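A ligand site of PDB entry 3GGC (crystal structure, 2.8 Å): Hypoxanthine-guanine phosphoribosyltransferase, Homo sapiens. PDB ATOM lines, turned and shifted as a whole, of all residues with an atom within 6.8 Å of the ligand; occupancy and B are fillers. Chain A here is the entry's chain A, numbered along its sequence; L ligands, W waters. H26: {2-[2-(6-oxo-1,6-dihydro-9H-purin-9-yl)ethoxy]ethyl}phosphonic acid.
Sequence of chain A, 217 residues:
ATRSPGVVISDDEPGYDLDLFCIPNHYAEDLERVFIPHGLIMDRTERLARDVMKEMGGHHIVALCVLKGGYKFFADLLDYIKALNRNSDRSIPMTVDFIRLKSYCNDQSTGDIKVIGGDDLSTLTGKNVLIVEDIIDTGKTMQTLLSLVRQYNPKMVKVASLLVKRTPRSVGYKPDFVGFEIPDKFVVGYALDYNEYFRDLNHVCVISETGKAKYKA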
ATOM      1  N   LYS A  68     -24.607  20.135   3.575  1.00  0.00           N
ATOM      2  CA  LYS A  68     -24.402  21.529   3.206  1.00  0.00           C
ATOM      3  C   LYS A  68     -25.524  21.944   2.259  1.00  0.00           C
ATOM      4  O   LYS A  68     -26.580  22.380   2.705  1.00  0.00           O
ATOM      5  CB  LYS A  68     -23.021  21.759   2.569  1.00  0.00           C
ATOM      6  CG  LYS A  68     -21.911  22.021   3.577  1.00  0.00           C
ATOM      7  CD  LYS A  68     -21.107  20.771   3.890  1.00  0.00           C
ATOM      8  CE  LYS A  68     -19.866  20.652   3.007  1.00  0.00           C
ATOM      9  NZ  LYS A  68     -20.154  20.206   1.613  1.00  0.00           N
ATOM     10  N   THR A 110     -13.077  27.848   7.275  1.00  0.00           N
ATOM     11  CA  THR A 110     -14.022  26.735   7.144  1.00  0.00           C
ATOM     12  C   THR A 110     -14.139  25.937   8.434  1.00  0.00           C
ATOM     13  O   THR A 110     -15.141  25.243   8.661  1.00  0.00           O
ATOM     14  CB  THR A 110     -13.595  25.772   6.010  1.00  0.00           C
ATOM     15  OG1 THR A 110     -12.609  26.411   5.183  1.00  0.00           O
ATOM     16  CG2 THR A 110     -14.793  25.357   5.168  1.00  0.00           C
ATOM     17  N   GLY A 111     -13.118  26.022   9.273  1.00  0.00           N
ATOM     18  CA  GLY A 111     -13.049  25.253  10.515  1.00  0.00           C
ATOM     19  C   GLY A 111     -14.154  25.619  11.482  1.00  0.00           C
ATOM     20  O   GLY A 111     -14.590  24.800  12.285  1.00  0.00           O
ATOM     21  N   GLU A 133     -19.413  12.829   3.770  1.00  0.00           N
ATOM     22  CA  GLU A 133     -19.131  14.162   3.255  1.00  0.00           C
ATOM     23  C   GLU A 133     -18.821  14.043   1.768  1.00  0.00           C
ATOM     24  O   GLU A 133     -18.342  12.998   1.314  1.00  0.00           O
ATOM     25  CB  GLU A 133     -17.930  14.755   4.003  1.00  0.00           C
ATOM     26  CG  GLU A 133     -17.453  16.103   3.502  1.00  0.00           C
ATOM     27  CD  GLU A 133     -18.438  17.221   3.776  1.00  0.00           C
ATOM     28  OE1 GLU A 133     -18.062  18.192   4.454  1.00  0.00           O
ATOM     29  OE2 GLU A 133     -19.598  17.116   3.309  1.00  0.00           O
ATOM     30  N   ASP A 134     -19.097  15.098   1.002  1.00  0.00           N
ATOM     31  CA  ASP A 134     -18.907  15.044  -0.448  1.00  0.00           C
ATOM     32  C   ASP A 134     -17.513  15.466  -0.913  1.00  0.00           C
ATOM     33  O   ASP A 134     -16.942  14.866  -1.835  1.00  0.00           O
ATOM     34  CB  ASP A 134     -20.002  15.834  -1.182  1.00  0.00           C
ATOM     35  CG  ASP A 134     -20.181  17.243  -0.635  1.00  0.00           C
ATOM     36  OD1 ASP A 134     -19.213  17.824  -0.082  1.00  0.00           O
ATOM     37  OD2 ASP A 134     -21.303  17.775  -0.744  1.00  0.00           O
ATOM     38  N   ILE A 135     -16.973  16.505  -0.289  1.00  0.00           N
ATOM     39  CA  ILE A 135     -15.652  16.989  -0.659  1.00  0.00           C
ATOM     40  C   ILE A 135     -14.914  17.455   0.576  1.00  0.00           C
ATOM     41  O   ILE A 135     -15.491  18.098   1.454  1.00  0.00           O
ATOM     42  CB  ILE A 135     -15.749  18.151  -1.657  1.00  0.00           C
ATOM     43  CG1 ILE A 135     -14.348  18.650  -2.027  1.00  0.00           C
ATOM     44  CG2 ILE A 135     -16.605  19.268  -1.091  1.00  0.00           C
ATOM     45  CD1 ILE A 135     -14.269  19.258  -3.407  1.00  0.00           C
ATOM     46  N   ILE A 136     -13.639  17.111   0.652  1.00  0.00           N
ATOM     47  CA  ILE A 136     -12.758  17.632   1.689  1.00  0.00           C
ATOM     48  C   ILE A 136     -11.674  18.447   1.007  1.00  0.00           C
ATOM     49  O   ILE A 136     -11.033  17.996   0.058  1.00  0.00           O
ATOM     50  CB  ILE A 136     -12.113  16.517   2.533  1.00  0.00           C
ATOM     51  CG1 ILE A 136     -13.178  15.795   3.374  1.00  0.00           C
ATOM     52  CG2 ILE A 136     -11.028  17.091   3.444  1.00  0.00           C
ATOM     53  CD1 ILE A 136     -12.634  14.662   4.206  1.00  0.00           C
ATOM     54  N   ASP A 137     -11.492  19.675   1.496  1.00  0.00           N
ATOM     55  CA  ASP A 137     -10.533  20.595   0.921  1.00  0.00           C
ATOM     56  C   ASP A 137      -9.399  20.874   1.906  1.00  0.00           C
ATOM     57  O   ASP A 137      -8.428  20.130   1.965  1.00  0.00           O
ATOM     58  CB  ASP A 137     -11.234  21.889   0.500  1.00  0.00           C
ATOM     59  CG  ASP A 137     -10.354  22.790  -0.333  1.00  0.00           C
ATOM     60  OD1 ASP A 137      -9.461  22.260  -1.043  1.00  0.00           O
ATOM     61  OD2 ASP A 137     -10.536  24.021  -0.280  1.00  0.00           O
ATOM     62  N   THR A 138      -9.519  21.937   2.692  1.00  0.00           N
ATOM     63  CA  THR A 138      -8.488  22.247   3.678  1.00  0.00           C
ATOM     64  C   THR A 138      -8.544  21.276   4.854  1.00  0.00           C
ATOM     65  O   THR A 138      -7.556  21.069   5.556  1.00  0.00           O
ATOM     66  CB  THR A 138      -8.607  23.699   4.202  1.00  0.00           C
ATOM     67  OG1 THR A 138      -9.845  23.861   4.903  1.00  0.00           O
ATOM     68  CG2 THR A 138      -8.533  24.686   3.054  1.00  0.00           C
ATOM     69  N   GLY A 139      -9.721  20.677   5.064  1.00  0.00           N
ATOM     70  CA  GLY A 139      -9.894  19.667   6.091  1.00  0.00           C
ATOM     71  C   GLY A 139     -10.340  20.247   7.419  1.00  0.00           C
ATOM     72  O   GLY A 139     -10.495  19.523   8.400  1.00  0.00           O
ATOM     73  N   LYS A 140     -10.549  21.565   7.443  1.00  0.00           N
ATOM     74  CA  LYS A 140     -10.918  22.247   8.680  1.00  0.00           C
ATOM     75  C   LYS A 140     -12.338  21.956   9.156  1.00  0.00           C
ATOM     76  O   LYS A 140     -12.564  21.729  10.348  1.00  0.00           O
ATOM     77  CB  LYS A 140     -10.731  23.761   8.507  1.00  0.00           C
ATOM     78  CG  LYS A 140      -9.283  24.185   8.423  1.00  0.00           C
ATOM     79  CD  LYS A 140      -9.180  25.670   8.148  1.00  0.00           C
ATOM     80  CE  LYS A 140      -7.742  26.093   7.951  1.00  0.00           C
ATOM     81  NZ  LYS A 140      -7.625  27.252   7.019  1.00  0.00           N
ATOM     82  N   THR A 141     -13.297  21.960   8.234  1.00  0.00           N
ATOM     83  CA  THR A 141     -14.681  21.685   8.578  1.00  0.00           C
ATOM     84  C   THR A 141     -14.780  20.361   9.309  1.00  0.00           C
ATOM     85  O   THR A 141     -15.366  20.266  10.395  1.00  0.00           O
ATOM     86  CB  THR A 141     -15.565  21.617   7.330  1.00  0.00           C
ATOM     87  OG1 THR A 141     -15.743  22.946   6.799  1.00  0.00           O
ATOM     88  CG2 THR A 141     -16.923  21.031   7.670  1.00  0.00           C
ATOM     89  N   MET A 142     -14.202  19.329   8.708  1.00  0.00           N
ATOM     90  CA  MET A 142     -14.292  17.986   9.241  1.00  0.00           C
ATOM     91  C   MET A 142     -13.657  17.869  10.620  1.00  0.00           C
ATOM     92  O   MET A 142     -14.294  17.402  11.575  1.00  0.00           O
ATOM     93  CB  MET A 142     -13.661  16.985   8.286  1.00  0.00           C
ATOM     94  CG  MET A 142     -14.036  15.547   8.592  1.00  0.00           C
ATOM     95  SD  MET A 142     -15.820  15.370   8.738  1.00  0.00           S
ATOM     96  CE  MET A 142     -16.353  15.887   7.100  1.00  0.00           C
ATOM     97  N   LEU A 163     -14.674  13.075  -2.303  1.00  0.00           N
ATOM     98  CA  LEU A 163     -13.551  13.788  -2.879  1.00  0.00           C
ATOM     99  C   LEU A 163     -12.642  14.371  -1.809  1.00  0.00           C
ATOM    100  O   LEU A 163     -13.094  15.064  -0.890  1.00  0.00           O
ATOM    101  CB  LEU A 163     -14.049  14.927  -3.759  1.00  0.00           C
ATOM    102  CG  LEU A 163     -15.122  14.630  -4.811  1.00  0.00           C
ATOM    103  CD1 LEU A 163     -15.632  15.926  -5.435  1.00  0.00           C
ATOM    104  CD2 LEU A 163     -14.560  13.692  -5.873  1.00  0.00           C
ATOM    105  N   LYS A 165      -9.278  16.729  -1.812  1.00  0.00           N
ATOM    106  CA  LYS A 165      -8.531  17.596  -2.712  1.00  0.00           C
ATOM    107  C   LYS A 165      -7.067  17.639  -2.312  1.00  0.00           C
ATOM    108  O   LYS A 165      -6.744  17.786  -1.129  1.00  0.00           O
ATOM    109  CB  LYS A 165      -9.140  18.996  -2.687  1.00  0.00           C
ATOM    110  CG  LYS A 165      -8.951  19.809  -3.941  1.00  0.00           C
ATOM    111  CD  LYS A 165     -10.253  20.538  -4.255  1.00  0.00           C
ATOM    112  CE  LYS A 165     -10.003  21.945  -4.779  1.00  0.00           C
ATOM    113  NZ  LYS A 165     -11.300  22.672  -4.929  1.00  0.00           N
ATOM    114  N   ARG A 169      -2.937  23.905   1.102  1.00  0.00           N
ATOM    115  CA  ARG A 169      -3.803  24.507   2.111  1.00  0.00           C
ATOM    116  C   ARG A 169      -4.392  23.473   3.079  1.00  0.00           C
ATOM    117  O   ARG A 169      -5.065  23.824   4.049  1.00  0.00           O
ATOM    118  CB  ARG A 169      -4.921  25.319   1.433  1.00  0.00           C
ATOM    119  CG  ARG A 169      -4.460  26.671   0.877  1.00  0.00           C
ATOM    120  CD  ARG A 169      -5.353  27.177  -0.260  1.00  0.00           C
ATOM    121  NE  ARG A 169      -6.749  26.830  -0.052  1.00  0.00           N
ATOM    122  CZ  ARG A 169      -7.408  25.895  -0.742  1.00  0.00           C
ATOM    123  NH1 ARG A 169      -6.796  25.215  -1.700  1.00  0.00           N
ATOM    124  NH2 ARG A 169      -8.683  25.653  -0.471  1.00  0.00           N
ATOM    125  N   ILE A 182      -8.212  14.232  -5.896  1.00  0.00           N
ATOM    126  CA  ILE A 182      -8.263  15.054  -7.112  1.00  0.00           C
ATOM    127  C   ILE A 182      -7.312  16.238  -7.045  1.00  0.00           C
ATOM    128  O   ILE A 182      -6.879  16.628  -5.954  1.00  0.00           O
ATOM    129  CB  ILE A 182      -9.686  15.580  -7.328  1.00  0.00           C
ATOM    130  CG1 ILE A 182     -10.143  16.355  -6.083  1.00  0.00           C
ATOM    131  CG2 ILE A 182     -10.628  14.441  -7.627  1.00  0.00           C
ATOM    132  CD1 ILE A 182     -11.239  17.363  -6.354  1.00  0.00           C
ATOM    133  N   LYS A 185      -8.152  21.999  -8.004  1.00  0.00           N
ATOM    134  CA  LYS A 185      -8.957  22.860  -8.880  1.00  0.00           C
ATOM    135  C   LYS A 185     -10.400  22.873  -8.394  1.00  0.00           C
ATOM    136  O   LYS A 185     -10.853  21.909  -7.785  1.00  0.00           O
ATOM    137  CB  LYS A 185      -8.881  22.368 -10.332  1.00  0.00           C
ATOM    138  CG  LYS A 185      -7.572  22.721 -11.031  1.00  0.00           C
ATOM    139  CD  LYS A 185      -7.364  21.870 -12.276  1.00  0.00           C
ATOM    140  CE  LYS A 185      -6.012  22.160 -12.923  1.00  0.00           C
ATOM    141  NZ  LYS A 185      -5.724  21.242 -14.071  1.00  0.00           N
ATOM    142  N   PHE A 186     -11.120  23.954  -8.659  1.00  0.00           N
ATOM    143  CA  PHE A 186     -12.489  24.079  -8.147  1.00  0.00           C
ATOM    144  C   PHE A 186     -13.514  23.346  -9.019  1.00  0.00           C
ATOM    145  O   PHE A 186     -13.753  23.715 -10.173  1.00  0.00           O
ATOM    146  CB  PHE A 186     -12.888  25.554  -7.988  1.00  0.00           C
ATOM    147  CG  PHE A 186     -14.160  25.754  -7.207  1.00  0.00           C
ATOM    148  CD1 PHE A 186     -14.116  26.119  -5.871  1.00  0.00           C
ATOM    149  CD2 PHE A 186     -15.396  25.582  -7.808  1.00  0.00           C
ATOM    150  CE1 PHE A 186     -15.286  26.306  -5.153  1.00  0.00           C
ATOM    151  CE2 PHE A 186     -16.566  25.768  -7.091  1.00  0.00           C
ATOM    152  CZ  PHE A 186     -16.511  26.130  -5.763  1.00  0.00           C
ATOM    153  N   VAL A 187     -14.126  22.301  -8.458  1.00  0.00           N
ATOM    154  CA  VAL A 187     -15.004  21.414  -9.223  1.00  0.00           C
ATOM    155  C   VAL A 187     -16.500  21.562  -8.894  1.00  0.00           C
ATOM    156  O   VAL A 187     -16.871  21.928  -7.773  1.00  0.00           O
ATOM    157  CB  VAL A 187     -14.594  19.935  -9.040  1.00  0.00           C
ATOM    158  CG1 VAL A 187     -13.231  19.689  -9.651  1.00  0.00           C
ATOM    159  CG2 VAL A 187     -14.596  19.556  -7.571  1.00  0.00           C
ATOM    160  N   VAL A 188     -17.344  21.289  -9.885  1.00  0.00           N
ATOM    161  CA  VAL A 188     -18.788  21.292  -9.679  1.00  0.00           C
ATOM    162  C   VAL A 188     -19.398  20.026 -10.293  1.00  0.00           C
ATOM    163  O   VAL A 188     -18.753  19.352 -11.089  1.00  0.00           O
ATOM    164  CB  VAL A 188     -19.451  22.528 -10.327  1.00  0.00           C
ATOM    165  CG1 VAL A 188     -18.926  23.810  -9.673  1.00  0.00           C
ATOM    166  CG2 VAL A 188     -19.190  22.544 -11.821  1.00  0.00           C
ATOM    167  N   LEU A 192     -21.915  18.634  -5.947  1.00  0.00           N
ATOM    168  CA  LEU A 192     -21.500  20.002  -5.671  1.00  0.00           C
ATOM    169  C   LEU A 192     -22.189  20.986  -6.611  1.00  0.00           C
ATOM    170  O   LEU A 192     -21.940  20.985  -7.818  1.00  0.00           O
ATOM    171  CB  LEU A 192     -19.988  20.121  -5.784  1.00  0.00           C
ATOM    172  CG  LEU A 192     -19.223  19.149  -4.881  1.00  0.00           C
ATOM    173  CD1 LEU A 192     -17.729  19.305  -5.073  1.00  0.00           C
ATOM    174  CD2 LEU A 192     -19.606  19.370  -3.416  1.00  0.00           C
ATOM    175  N   ASP A 193     -23.065  21.810  -6.055  1.00  0.00           N
ATOM    176  CA  ASP A 193     -23.720  22.884  -6.795  1.00  0.00           C
ATOM    177  C   ASP A 193     -22.893  24.150  -6.667  1.00  0.00           C
ATOM    178  O   ASP A 193     -22.018  24.244  -5.802  1.00  0.00           O
ATOM    179  CB  ASP A 193     -25.119  23.159  -6.247  1.00  0.00           C
ATOM    180  CG  ASP A 193     -25.096  24.012  -4.987  1.00  0.00           C
ATOM    181  OD1 ASP A 193     -24.783  23.473  -3.898  1.00  0.00           O
ATOM    182  OD2 ASP A 193     -25.379  25.223  -5.082  1.00  0.00           O
ATOM    183  N   TYR A 194     -23.164  25.125  -7.523  1.00  0.00           N
ATOM    184  CA  TYR A 194     -22.504  26.412  -7.444  1.00  0.00           C
ATOM    185  C   TYR A 194     -23.567  27.489  -7.474  1.00  0.00           C
ATOM    186  O   TYR A 194     -24.237  27.690  -8.494  1.00  0.00           O
ATOM    187  CB  TYR A 194     -21.524  26.569  -8.614  1.00  0.00           C
ATOM    188  CG  TYR A 194     -20.691  27.827  -8.567  1.00  0.00           C
ATOM    189  CD1 TYR A 194     -19.580  27.923  -7.737  1.00  0.00           C
ATOM    190  CD2 TYR A 194     -21.012  28.920  -9.367  1.00  0.00           C
ATOM    191  CE1 TYR A 194     -18.822  29.074  -7.708  1.00  0.00           C
ATOM    192  CE2 TYR A 194     -20.254  30.071  -9.338  1.00  0.00           C
ATOM    193  CZ  TYR A 194     -19.159  30.148  -8.508  1.00  0.00           C
ATOM    194  OH  TYR A 194     -18.398  31.292  -8.473  1.00  0.00           O
HETATM  195  OAD H26 L   1     -12.200  23.116   3.123  1.00  0.00           O
HETATM  196  PAT H26 L   1     -12.921  22.107   3.981  1.00  0.00           P
HETATM  197  OAE H26 L   1     -13.338  22.632   5.342  1.00  0.00           O
HETATM  198  OAC H26 L   1     -12.258  20.751   4.005  1.00  0.00           O
HETATM  199  CAJ H26 L   1     -14.499  21.850   3.125  1.00  0.00           C
HETATM  200  CAH H26 L   1     -14.651  22.982   2.129  1.00  0.00           C
HETATM  201  OAN H26 L   1     -15.269  22.481   0.948  1.00  0.00           O
HETATM  202  CAG H26 L   1     -16.456  23.211   0.634  1.00  0.00           C
HETATM  203  CAI H26 L   1     -16.131  24.375  -0.301  1.00  0.00           C
HETATM  204  N9  H26 L   1     -15.298  23.928  -1.417  1.00  0.00           N
HETATM  205  C8  H26 L   1     -13.960  23.818  -1.406  1.00  0.00           C
HETATM  206  N7  H26 L   1     -13.534  23.383  -2.607  1.00  0.00           N
HETATM  207  C4  H26 L   1     -15.734  23.548  -2.628  1.00  0.00           C
HETATM  208  C5  H26 L   1     -14.626  23.203  -3.385  1.00  0.00           C
HETATM  209  N3  H26 L   1     -16.969  23.458  -3.190  1.00  0.00           N
HETATM  210  C2  H26 L   1     -17.115  23.032  -4.456  1.00  0.00           C
HETATM  211  N1  H26 L   1     -16.050  22.696  -5.200  1.00  0.00           N
HETATM  212  C6  H26 L   1     -14.793  22.763  -4.693  1.00  0.00           C
HETATM  213  O6  H26 L   1     -13.707  22.419  -5.454  1.00  0.00           O
HETATM  214  O   HOH W   1     -13.229  19.784   6.190  1.00  0.00           O
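The side-chain hydroxyl (OG1) of Thr 141 sits at hydrogen-bond distance from the backbone carbonyl oxygen (O) of Thr 110, at 3.0 Å.
The backbone NH (N) of Ile 136 is in hydrogen-bond range of the backbone carbonyl oxygen (O) of Leu 163, 2.6 Å away.
The side-chain hydroxyl (OG1) of Thr 138 lies close to the backbone NH (N) of Lys 140 (3.5 Å).
O of Ile 136 lies within hydrogen-bond range of N of Lys 165, 2.9 Å away.
The side-chain amino group (NZ) of Lys 165 sits at hydrogen-bond distance from the backbone carbonyl oxygen (O) of Lys 185.
OD2 of Asp 137 is in salt-bridge range of NH2 of Arg 169.
OAE of the ligand sits at hydrogen-bond distance from OG1 of Thr 141, at 2.8 Å.
N of Asp 137 is in hydrogen-bond range of OAC of the ligand, 2.8 Å away.
An oxygen (OAE) of the ligand is in hydrogen-bond range of the backbone NH (N) of Thr 141 (3.0 Å).
N of Gly 139 is in hydrogen-bond range of OAC of the ligand, 2.8 Å away.
A nitrogen (N1) of the ligand is in hydrogen-bond range of the backbone carbonyl oxygen (O) of Val 187 (2.8 Å).
An oxygen (O6) of the ligand is in hydrogen-bond range of the side-chain amino group (NZ) of Lys 165 (2.5 Å).
O6 of the ligand sits at hydrogen-bond distance from N of Val 187.
The backbone NH of Thr 138 sits at hydrogen-bond distance from an oxygen (OAD) of the ligand.
OG1 of Thr 138 sits at hydrogen-bond distance from OAD of the ligand (3.0 Å).
Thr 110 touches the ligand (CG2 to OAE, 3.1 Å).
Ile 135 touches the ligand.
C of Ile 136 touches OAC of the ligand (3.8 Å).
N of Lys 140 touches OAE of the ligand (3.7 Å).
O of Lys 185 touches O6 of the ligand, at 3.7 Å.
CA of Phe 186 touches O6 of the ligand (3.4 Å).
Leu 192 touches the ligand.
Hydrophobic or aromatic side chains within 4 Å of the ligand: Ile 135, Ile 136, Phe 186, Val 187 and Leu 192.
Of the 24 residues printed, 13 come within 4 Å of the ligand.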
